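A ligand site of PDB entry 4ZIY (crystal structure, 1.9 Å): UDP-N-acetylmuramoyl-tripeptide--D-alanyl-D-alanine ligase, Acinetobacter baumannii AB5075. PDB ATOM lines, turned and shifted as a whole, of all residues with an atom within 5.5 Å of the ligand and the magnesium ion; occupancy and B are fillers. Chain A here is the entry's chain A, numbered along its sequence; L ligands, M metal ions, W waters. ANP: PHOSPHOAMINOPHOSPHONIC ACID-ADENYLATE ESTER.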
ATOM      1  N   GLY A 129     -13.150 -15.345  33.548  1.00  0.00           N
ATOM      2  CA  GLY A 129     -13.337 -14.494  32.392  1.00  0.00           C
ATOM      3  C   GLY A 129     -13.902 -15.337  31.286  1.00  0.00           C
ATOM      4  O   GLY A 129     -13.906 -16.567  31.385  1.00  0.00           O
ATOM      5  N   SER A 130     -14.423 -14.711  30.235  1.00  0.00           N
ATOM      6  CA  SER A 130     -14.962 -15.493  29.129  1.00  0.00           C
ATOM      7  C   SER A 130     -13.824 -16.028  28.233  1.00  0.00           C
ATOM      8  O   SER A 130     -13.907 -17.136  27.709  1.00  0.00           O
ATOM      9  CB  SER A 130     -15.943 -14.661  28.317  1.00  0.00           C
ATOM     10  OG  SER A 130     -17.119 -14.380  29.076  1.00  0.00           O
ATOM     11  N   SER A 131     -12.771 -15.228  28.081  1.00  0.00           N
ATOM     12  CA  SER A 131     -11.624 -15.638  27.277  1.00  0.00           C
ATOM     13  C   SER A 131     -10.330 -15.238  27.953  1.00  0.00           C
ATOM     14  O   SER A 131     -10.295 -14.329  28.790  1.00  0.00           O
ATOM     15  CB  SER A 131     -11.694 -15.027  25.873  1.00  0.00           C
ATOM     16  OG  SER A 131     -12.871 -15.440  25.209  1.00  0.00           O
ATOM     17  N   GLY A 132      -9.246 -15.929  27.587  1.00  0.00           N
ATOM     18  CA  GLY A 132      -7.931 -15.603  28.120  1.00  0.00           C
ATOM     19  C   GLY A 132      -7.561 -16.156  29.491  1.00  0.00           C
ATOM     20  O   GLY A 132      -6.486 -15.839  29.995  1.00  0.00           O
ATOM     21  N   LYS A 133      -8.428 -16.981  30.101  1.00  0.00           N
ATOM     22  CA  LYS A 133      -8.123 -17.493  31.453  1.00  0.00           C
ATOM     23  C   LYS A 133      -6.845 -18.326  31.484  1.00  0.00           C
ATOM     24  O   LYS A 133      -5.941 -18.097  32.307  1.00  0.00           O
ATOM     25  CB  LYS A 133      -9.289 -18.362  31.986  1.00  0.00           C
ATOM     26  CG  LYS A 133     -10.600 -17.622  32.224  1.00  0.00           C
ATOM     27  CD  LYS A 133     -11.698 -18.523  32.841  1.00  0.00           C
ATOM     28  CE  LYS A 133     -12.118 -19.687  31.918  1.00  0.00           C
ATOM     29  NZ  LYS A 133     -12.772 -19.238  30.654  1.00  0.00           N
ATOM     30  N   THR A 134      -6.778 -19.288  30.587  1.00  0.00           N
ATOM     31  CA  THR A 134      -5.667 -20.235  30.581  1.00  0.00           C
ATOM     32  C   THR A 134      -4.373 -19.518  30.237  1.00  0.00           C
ATOM     33  O   THR A 134      -3.348 -19.739  30.871  1.00  0.00           O
ATOM     34  CB  THR A 134      -5.945 -21.375  29.589  1.00  0.00           C
ATOM     35  OG1 THR A 134      -6.981 -22.211  30.110  1.00  0.00           O
ATOM     36  CG2 THR A 134      -4.678 -22.206  29.347  1.00  0.00           C
ATOM     37  N   THR A 135      -4.420 -18.644  29.243  1.00  0.00           N
ATOM     38  CA  THR A 135      -3.206 -17.925  28.823  1.00  0.00           C
ATOM     39  C   THR A 135      -2.714 -17.015  29.947  1.00  0.00           C
ATOM     40  O   THR A 135      -1.521 -16.969  30.253  1.00  0.00           O
ATOM     41  CB  THR A 135      -3.469 -17.120  27.548  1.00  0.00           C
ATOM     42  OG1 THR A 135      -3.793 -18.026  26.488  1.00  0.00           O
ATOM     43  CG2 THR A 135      -2.237 -16.301  27.149  1.00  0.00           C
ATOM     44  N   THR A 136      -3.639 -16.284  30.588  1.00  0.00           N
ATOM     45  CA  THR A 136      -3.249 -15.415  31.707  1.00  0.00           C
ATOM     46  C   THR A 136      -2.716 -16.226  32.878  1.00  0.00           C
ATOM     47  O   THR A 136      -1.758 -15.843  33.542  1.00  0.00           O
ATOM     48  CB  THR A 136      -4.445 -14.524  32.161  1.00  0.00           C
ATOM     49  OG1 THR A 136      -4.927 -13.773  31.035  1.00  0.00           O
ATOM     50  CG2 THR A 136      -4.028 -13.536  33.262  1.00  0.00           C
ATOM     51  N   GLY A 155      -4.897 -28.033  32.667  1.00  0.00           N
ATOM     52  CA  GLY A 155      -5.963 -28.225  31.686  1.00  0.00           C
ATOM     53  C   GLY A 155      -7.300 -27.574  32.031  1.00  0.00           C
ATOM     54  O   GLY A 155      -7.345 -26.403  32.400  1.00  0.00           O
ATOM     55  N   ASN A 158     -11.401 -26.795  36.235  1.00  0.00           N
ATOM     56  CA  ASN A 158     -11.753 -25.450  36.694  1.00  0.00           C
ATOM     57  C   ASN A 158     -13.206 -25.315  37.126  1.00  0.00           C
ATOM     58  O   ASN A 158     -13.703 -24.201  37.298  1.00  0.00           O
ATOM     59  CB  ASN A 158     -11.411 -24.422  35.588  1.00  0.00           C
ATOM     60  CG  ASN A 158     -12.270 -24.581  34.333  1.00  0.00           C
ATOM     61  OD1 ASN A 158     -13.285 -25.265  34.328  1.00  0.00           O
ATOM     62  ND2 ASN A 158     -11.848 -23.936  33.244  1.00  0.00           N
ATOM     63  N   GLU A 180      -7.629 -21.168  38.060  1.00  0.00           N
ATOM     64  CA  GLU A 180      -8.596 -20.806  37.033  1.00  0.00           C
ATOM     65  C   GLU A 180      -9.989 -21.312  37.433  1.00  0.00           C
ATOM     66  O   GLU A 180     -10.154 -22.501  37.768  1.00  0.00           O
ATOM     67  CB  GLU A 180      -8.195 -21.407  35.699  1.00  0.00           C
ATOM     68  CG  GLU A 180      -9.189 -21.193  34.584  1.00  0.00           C
ATOM     69  CD  GLU A 180      -8.681 -21.773  33.258  1.00  0.00           C
ATOM     70  OE1 GLU A 180      -7.447 -21.861  33.064  1.00  0.00           O
ATOM     71  OE2 GLU A 180      -9.513 -22.127  32.420  1.00  0.00           O
ATOM     72  N   ASN A 205     -12.717 -10.507  31.387  1.00  0.00           N
ATOM     73  CA  ASN A 205     -13.655  -9.939  30.431  1.00  0.00           C
ATOM     74  C   ASN A 205     -14.998 -10.646  30.523  1.00  0.00           C
ATOM     75  O   ASN A 205     -15.063 -11.743  31.069  1.00  0.00           O
ATOM     76  CB  ASN A 205     -13.119 -10.070  28.989  1.00  0.00           C
ATOM     77  CG  ASN A 205     -12.561 -11.456  28.721  1.00  0.00           C
ATOM     78  OD1 ASN A 205     -13.309 -12.428  28.643  1.00  0.00           O
ATOM     79  ND2 ASN A 205     -11.234 -11.550  28.602  1.00  0.00           N
ATOM     80  N   HIS A 300      -4.819  -9.535  21.697  1.00  0.00           N
ATOM     81  CA  HIS A 300      -5.512 -10.149  22.834  1.00  0.00           C
ATOM     82  C   HIS A 300      -4.508 -10.623  23.889  1.00  0.00           C
ATOM     83  O   HIS A 300      -4.758 -10.542  25.085  1.00  0.00           O
ATOM     84  CB  HIS A 300      -6.397 -11.322  22.372  1.00  0.00           C
ATOM     85  CG  HIS A 300      -5.631 -12.457  21.759  1.00  0.00           C
ATOM     86  ND1 HIS A 300      -4.718 -12.284  20.738  1.00  0.00           N
ATOM     87  CD2 HIS A 300      -5.653 -13.787  22.035  1.00  0.00           C
ATOM     88  CE1 HIS A 300      -4.212 -13.466  20.406  1.00  0.00           C
ATOM     89  NE2 HIS A 300      -4.765 -14.387  21.175  1.00  0.00           N
ATOM     90  N   ASN A 301      -3.352 -11.090  23.435  1.00  0.00           N
ATOM     91  CA  ASN A 301      -2.360 -11.587  24.383  1.00  0.00           C
ATOM     92  C   ASN A 301      -1.614 -10.450  25.094  1.00  0.00           C
ATOM     93  O   ASN A 301      -1.096 -10.649  26.188  1.00  0.00           O
ATOM     94  CB  ASN A 301      -1.396 -12.545  23.681  1.00  0.00           C
ATOM     95  CG  ASN A 301      -1.948 -13.953  23.584  1.00  0.00           C
ATOM     96  OD1 ASN A 301      -2.673 -14.405  24.481  1.00  0.00           O
ATOM     97  ND2 ASN A 301      -1.648 -14.648  22.485  1.00  0.00           N
ATOM     98  N   GLN A 303      -3.355  -7.820  26.042  1.00  0.00           N
ATOM     99  CA  GLN A 303      -4.357  -7.649  27.094  1.00  0.00           C
ATOM    100  C   GLN A 303      -4.182  -8.664  28.219  1.00  0.00           C
ATOM    101  O   GLN A 303      -4.285  -8.319  29.405  1.00  0.00           O
ATOM    102  CB  GLN A 303      -5.762  -7.770  26.512  1.00  0.00           C
ATOM    103  CG  GLN A 303      -6.194  -6.594  25.653  1.00  0.00           C
ATOM    104  CD  GLN A 303      -7.688  -6.626  25.380  1.00  0.00           C
ATOM    105  OE1 GLN A 303      -8.119  -6.957  24.275  1.00  0.00           O
ATOM    106  NE2 GLN A 303      -8.488  -6.281  26.389  1.00  0.00           N
ATOM    107  N   ASN A 304      -3.960  -9.926  27.862  1.00  0.00           N
ATOM    108  CA  ASN A 304      -3.737 -10.964  28.884  1.00  0.00           C
ATOM    109  C   ASN A 304      -2.482 -10.643  29.709  1.00  0.00           C
ATOM    110  O   ASN A 304      -2.464 -10.821  30.939  1.00  0.00           O
ATOM    111  CB  ASN A 304      -3.625 -12.352  28.248  1.00  0.00           C
ATOM    112  CG  ASN A 304      -4.931 -12.815  27.630  1.00  0.00           C
ATOM    113  OD1 ASN A 304      -6.010 -12.436  28.089  1.00  0.00           O
ATOM    114  ND2 ASN A 304      -4.842 -13.643  26.594  1.00  0.00           N
ATOM    115  N   GLY A 334      -2.161 -25.666  21.746  1.00  0.00           N
ATOM    116  CA  GLY A 334      -3.265 -25.305  20.884  1.00  0.00           C
ATOM    117  C   GLY A 334      -3.667 -23.836  20.967  1.00  0.00           C
ATOM    118  O   GLY A 334      -4.695 -23.449  20.414  1.00  0.00           O
ATOM    119  N   ARG A 335      -2.861 -23.039  21.656  1.00  0.00           N
ATOM    120  CA  ARG A 335      -3.059 -21.581  21.700  1.00  0.00           C
ATOM    121  C   ARG A 335      -1.915 -20.895  20.959  1.00  0.00           C
ATOM    122  O   ARG A 335      -0.906 -20.559  21.576  1.00  0.00           O
ATOM    123  CB  ARG A 335      -3.111 -21.053  23.140  1.00  0.00           C
ATOM    124  CG  ARG A 335      -4.439 -21.257  23.875  1.00  0.00           C
ATOM    125  CD  ARG A 335      -4.618 -22.692  24.329  1.00  0.00           C
ATOM    126  NE  ARG A 335      -5.596 -22.777  25.405  1.00  0.00           N
ATOM    127  CZ  ARG A 335      -5.820 -23.871  26.120  1.00  0.00           C
ATOM    128  NH1 ARG A 335      -5.127 -24.981  25.864  1.00  0.00           N
ATOM    129  NH2 ARG A 335      -6.730 -23.874  27.078  1.00  0.00           N
ATOM    130  N   ASP A 349      -3.484 -23.417  16.478  1.00  0.00           N
ATOM    131  CA  ASP A 349      -4.457 -22.642  17.229  1.00  0.00           C
ATOM    132  C   ASP A 349      -5.746 -23.459  17.358  1.00  0.00           C
ATOM    133  O   ASP A 349      -6.865 -22.927  17.344  1.00  0.00           O
ATOM    134  CB  ASP A 349      -4.737 -21.305  16.532  1.00  0.00           C
ATOM    135  CG  ASP A 349      -5.286 -20.263  17.478  1.00  0.00           C
ATOM    136  OD1 ASP A 349      -4.897 -20.286  18.664  1.00  0.00           O
ATOM    137  OD2 ASP A 349      -6.106 -19.432  17.031  1.00  0.00           O
ATOM    138  N   TYR A 351      -7.152 -25.264  19.760  1.00  0.00           N
ATOM    139  CA  TYR A 351      -7.846 -25.493  21.030  1.00  0.00           C
ATOM    140  C   TYR A 351      -9.355 -25.231  20.917  1.00  0.00           C
ATOM    141  O   TYR A 351     -10.148 -26.082  21.309  1.00  0.00           O
ATOM    142  CB  TYR A 351      -7.262 -24.620  22.157  1.00  0.00           C
ATOM    143  CG  TYR A 351      -8.109 -24.721  23.426  1.00  0.00           C
ATOM    144  CD1 TYR A 351      -8.152 -25.891  24.165  1.00  0.00           C
ATOM    145  CD2 TYR A 351      -8.888 -23.654  23.841  1.00  0.00           C
ATOM    146  CE1 TYR A 351      -8.943 -25.997  25.310  1.00  0.00           C
ATOM    147  CE2 TYR A 351      -9.685 -23.739  24.981  1.00  0.00           C
ATOM    148  CZ  TYR A 351      -9.698 -24.912  25.711  1.00  0.00           C
ATOM    149  OH  TYR A 351     -10.494 -24.996  26.833  1.00  0.00           O
ATOM    150  N   ASN A 352      -9.751 -24.085  20.383  1.00  0.00           N
ATOM    151  CA  ASN A 352     -11.182 -23.806  20.190  1.00  0.00           C
ATOM    152  C   ASN A 352     -11.431 -22.741  19.132  1.00  0.00           C
ATOM    153  O   ASN A 352     -10.482 -22.239  18.504  1.00  0.00           O
ATOM    154  CB  ASN A 352     -11.822 -23.395  21.523  1.00  0.00           C
ATOM    155  CG  ASN A 352     -11.416 -21.994  21.963  1.00  0.00           C
ATOM    156  OD1 ASN A 352     -10.470 -21.399  21.435  1.00  0.00           O
ATOM    157  ND2 ASN A 352     -12.110 -21.469  22.964  1.00  0.00           N
ATOM    158  N   SER A 357     -12.980 -15.041  17.118  1.00  0.00           N
ATOM    159  CA  SER A 357     -11.609 -15.530  17.229  1.00  0.00           C
ATOM    160  C   SER A 357     -11.115 -16.163  15.921  1.00  0.00           C
ATOM    161  O   SER A 357      -9.913 -16.149  15.628  1.00  0.00           O
ATOM    162  CB  SER A 357     -11.499 -16.534  18.368  1.00  0.00           C
ATOM    163  OG  SER A 357     -11.989 -17.800  17.984  1.00  0.00           O
ATOM    164  N   LYS A 456      -7.336 -24.314  12.942  1.00  0.00           N
ATOM    165  CA  LYS A 456      -8.243 -23.857  13.981  1.00  0.00           C
ATOM    166  C   LYS A 456      -9.665 -24.393  13.797  1.00  0.00           C
ATOM    167  O   LYS A 456     -10.146 -24.515  12.669  1.00  0.00           O
ATOM    168  CB  LYS A 456      -8.278 -22.335  14.041  1.00  0.00           C
ATOM    169  CG  LYS A 456      -9.056 -21.755  15.215  1.00  0.00           C
ATOM    170  CD  LYS A 456      -8.963 -20.241  15.247  1.00  0.00           C
ATOM    171  CE  LYS A 456      -9.549 -19.669  16.521  1.00  0.00           C
ATOM    172  NZ  LYS A 456      -8.800 -20.116  17.729  1.00  0.00           N
HETATM  173  PG  ANP L   1     -11.996 -21.847  28.329  1.00  0.00           P
HETATM  174  O1G ANP L   1     -12.289 -22.976  27.255  1.00  0.00           O
HETATM  175  O2G ANP L   1     -11.189 -22.451  29.547  1.00  0.00           O
HETATM  176  O3G ANP L   1     -13.251 -21.317  28.834  1.00  0.00           O
HETATM  177  PB  ANP L   1      -9.975 -19.704  28.299  1.00  0.00           P
HETATM  178  O1B ANP L   1      -9.126 -20.399  29.245  1.00  0.00           O
HETATM  179  O2B ANP L   1     -10.720 -18.498  28.947  1.00  0.00           O
HETATM  180  N3B ANP L   1     -11.068 -20.698  27.603  1.00  0.00           N
HETATM  181  PA  ANP L   1      -7.708 -19.380  26.512  1.00  0.00           P
HETATM  182  O1A ANP L   1      -6.582 -18.583  27.224  1.00  0.00           O
HETATM  183  O2A ANP L   1      -7.477 -20.849  26.499  1.00  0.00           O
HETATM  184  O3A ANP L   1      -9.095 -19.044  27.190  1.00  0.00           O
HETATM  185  O5' ANP L   1      -7.946 -18.773  25.044  1.00  0.00           O
HETATM  186  C5' ANP L   1      -8.754 -19.488  24.081  1.00  0.00           C
HETATM  187  C4' ANP L   1      -8.942 -18.605  22.875  1.00  0.00           C
HETATM  188  O4' ANP L   1      -9.622 -17.394  23.261  1.00  0.00           O
HETATM  189  C3' ANP L   1      -7.644 -18.132  22.228  1.00  0.00           C
HETATM  190  O3' ANP L   1      -7.156 -19.114  21.318  1.00  0.00           O
HETATM  191  C2' ANP L   1      -8.076 -16.845  21.540  1.00  0.00           C
HETATM  192  O2' ANP L   1      -8.709 -17.123  20.292  1.00  0.00           O
HETATM  193  C1' ANP L   1      -9.119 -16.296  22.519  1.00  0.00           C
HETATM  194  N9  ANP L   1      -8.617 -15.286  23.454  1.00  0.00           N
HETATM  195  C8  ANP L   1      -7.540 -15.398  24.286  1.00  0.00           C
HETATM  196  N7  ANP L   1      -7.381 -14.376  25.087  1.00  0.00           N
HETATM  197  C5  ANP L   1      -8.444 -13.530  24.770  1.00  0.00           C
HETATM  198  C6  ANP L   1      -8.860 -12.299  25.286  1.00  0.00           C
HETATM  199  N6  ANP L   1      -8.256 -11.666  26.298  1.00  0.00           N
HETATM  200  N1  ANP L   1      -9.956 -11.721  24.737  1.00  0.00           N
HETATM  201  C2  ANP L   1     -10.585 -12.358  23.741  1.00  0.00           C
HETATM  202  N3  ANP L   1     -10.289 -13.533  23.180  1.00  0.00           N
HETATM  203  C4  ANP L   1      -9.203 -14.077  23.742  1.00  0.00           C
HETATM  204 MG    MG M   1      -9.335 -22.377  30.272  1.00  0.00          MG
HETATM  205  O   HOH W   1      -9.101 -24.577  30.715  1.00  0.00           O
HETATM  206  O   HOH W   2     -12.892 -19.057  26.103  1.00  0.00           O
HETATM  207  O   HOH W   3      -7.513 -21.737  20.087  1.00  0.00           O
HETATM  208  O   HOH W   4      -9.202  -9.214  28.157  1.00  0.00           O
HETATM  209  O   HOH W   5      -7.276 -16.835  17.934  1.00  0.00           O
HETATM  210  O   HOH W   6      -4.395 -16.735  24.071  1.00  0.00           O
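The magnesium ion is bound by O2G of the ligand (2.0 Å), OE2 of Glu 180 (2.2 Å), O1B of the ligand (2.2 Å), water W1 (2.3 Å) and OG1 of Thr 134 (2.4 Å).
The magnesium ion has five donor atoms within binding distance.
The side-chain amino group of Lys 456 is in salt-bridge range of the side-chain carboxylate of Asp 349.
ND2 of Asn 158 lies close to OE2 of Glu 180.
The side-chain amino group (NZ) of Lys 133 sits at hydrogen-bond distance from the backbone carbonyl oxygen (O) of Gly 129.
The backbone carbonyl oxygen (O) of Asn 352 lies within hydrogen-bond range of the side-chain amino group (NZ) of Lys 456 (2.8 Å).
OD1 of Asn 304 lies close to OG1 of Thr 136, at 3.4 Å.
O of Gly 334 sits at hydrogen-bond distance from N of Tyr 351 (3.1 Å).
The side-chain hydroxyl (OG1) of Thr 134 lies close to the guanidinium group (NH2) of Arg 335, at 3.5 Å.
The backbone NH of Ser 131 lies within hydrogen-bond range of the side-chain amide oxygen of Asn 205.
Within 4 Å of the magnesium ion: Thr 134 and Glu 180.
The backbone NH (N) of Lys 133 lies within hydrogen-bond range of an oxygen (O2B) of the ligand (3.0 Å).
The backbone NH of Thr 135 sits at hydrogen-bond distance from an oxygen (O1A) of the ligand, 3.0 Å away.
The guanidinium group of Arg 335 is in salt-bridge range of an oxygen (O2A) of the ligand, at 2.9 Å.
The side-chain hydroxyl (OG1) of Thr 135 sits at hydrogen-bond distance from an oxygen (O1A) of the ligand.
The side-chain amide oxygen (OD1) of Asn 304 lies within hydrogen-bond range of a nitrogen (N6) of the ligand (3.0 Å).
The side-chain amino group of Lys 133 is in salt-bridge range of an oxygen (O2B) of the ligand (2.8 Å).
O1G of the ligand sits at hydrogen-bond distance from OH of Tyr 351, at 2.7 Å.
The backbone NH (N) of Thr 134 is in hydrogen-bond range of an oxygen (O1A) of the ligand, at 3.4 Å.
The backbone NH of Gly 132 is in hydrogen-bond range of an oxygen (O3A) of the ligand, at 3.1 Å.
Water W5 bridges an oxygen (O2') of the ligand (2.8 Å) and the side-chain carboxylate of Asp 349 (3.0 Å).
Water W2 bridges O of Ser 130 (2.7 Å) and N3B of the ligand (2.9 Å).
Water W3 lies within hydrogen-bond range of an oxygen (O3') of the ligand (2.9 Å), the backbone carbonyl oxygen (O) of Asp 349 (3.1 Å), the side-chain amino group (NZ) of Lys 456 (3.1 Å), the backbone NH (N) of Asn 352 (3.3 Å) and the backbone carbonyl oxygen (O) of Gly 334 (3.3 Å).
Water W6 bridges OG1 of Thr 135 and OD1 of Asn 301.
Ser 130 touches the ligand (O to O2B, 3.7 Å).
Ser 131 touches the ligand.
ND2 of Asn 205 touches N6 of the ligand, 3.8 Å away.
CD2 of His 300 touches C8 of the ligand, at 3.4 Å.
OD1 of Asp 349 touches O3' of the ligand, at 3.7 Å.
OD1 of Asn 352 touches C4' of the ligand, 3.5 Å away.
Ser 357 touches the ligand.
NZ of Lys 456 touches O2' of the ligand, at 3.9 Å.
16 residues have an atom within 4 Å of the ligand: Ser 130, Ser 131, Gly 132, Lys 133, Thr 134, Thr 135, Glu 180, Asn 205, His 300, Asn 304, Arg 335, Asp 349, Tyr 351, Asn 352, Ser 357 and Lys 456.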
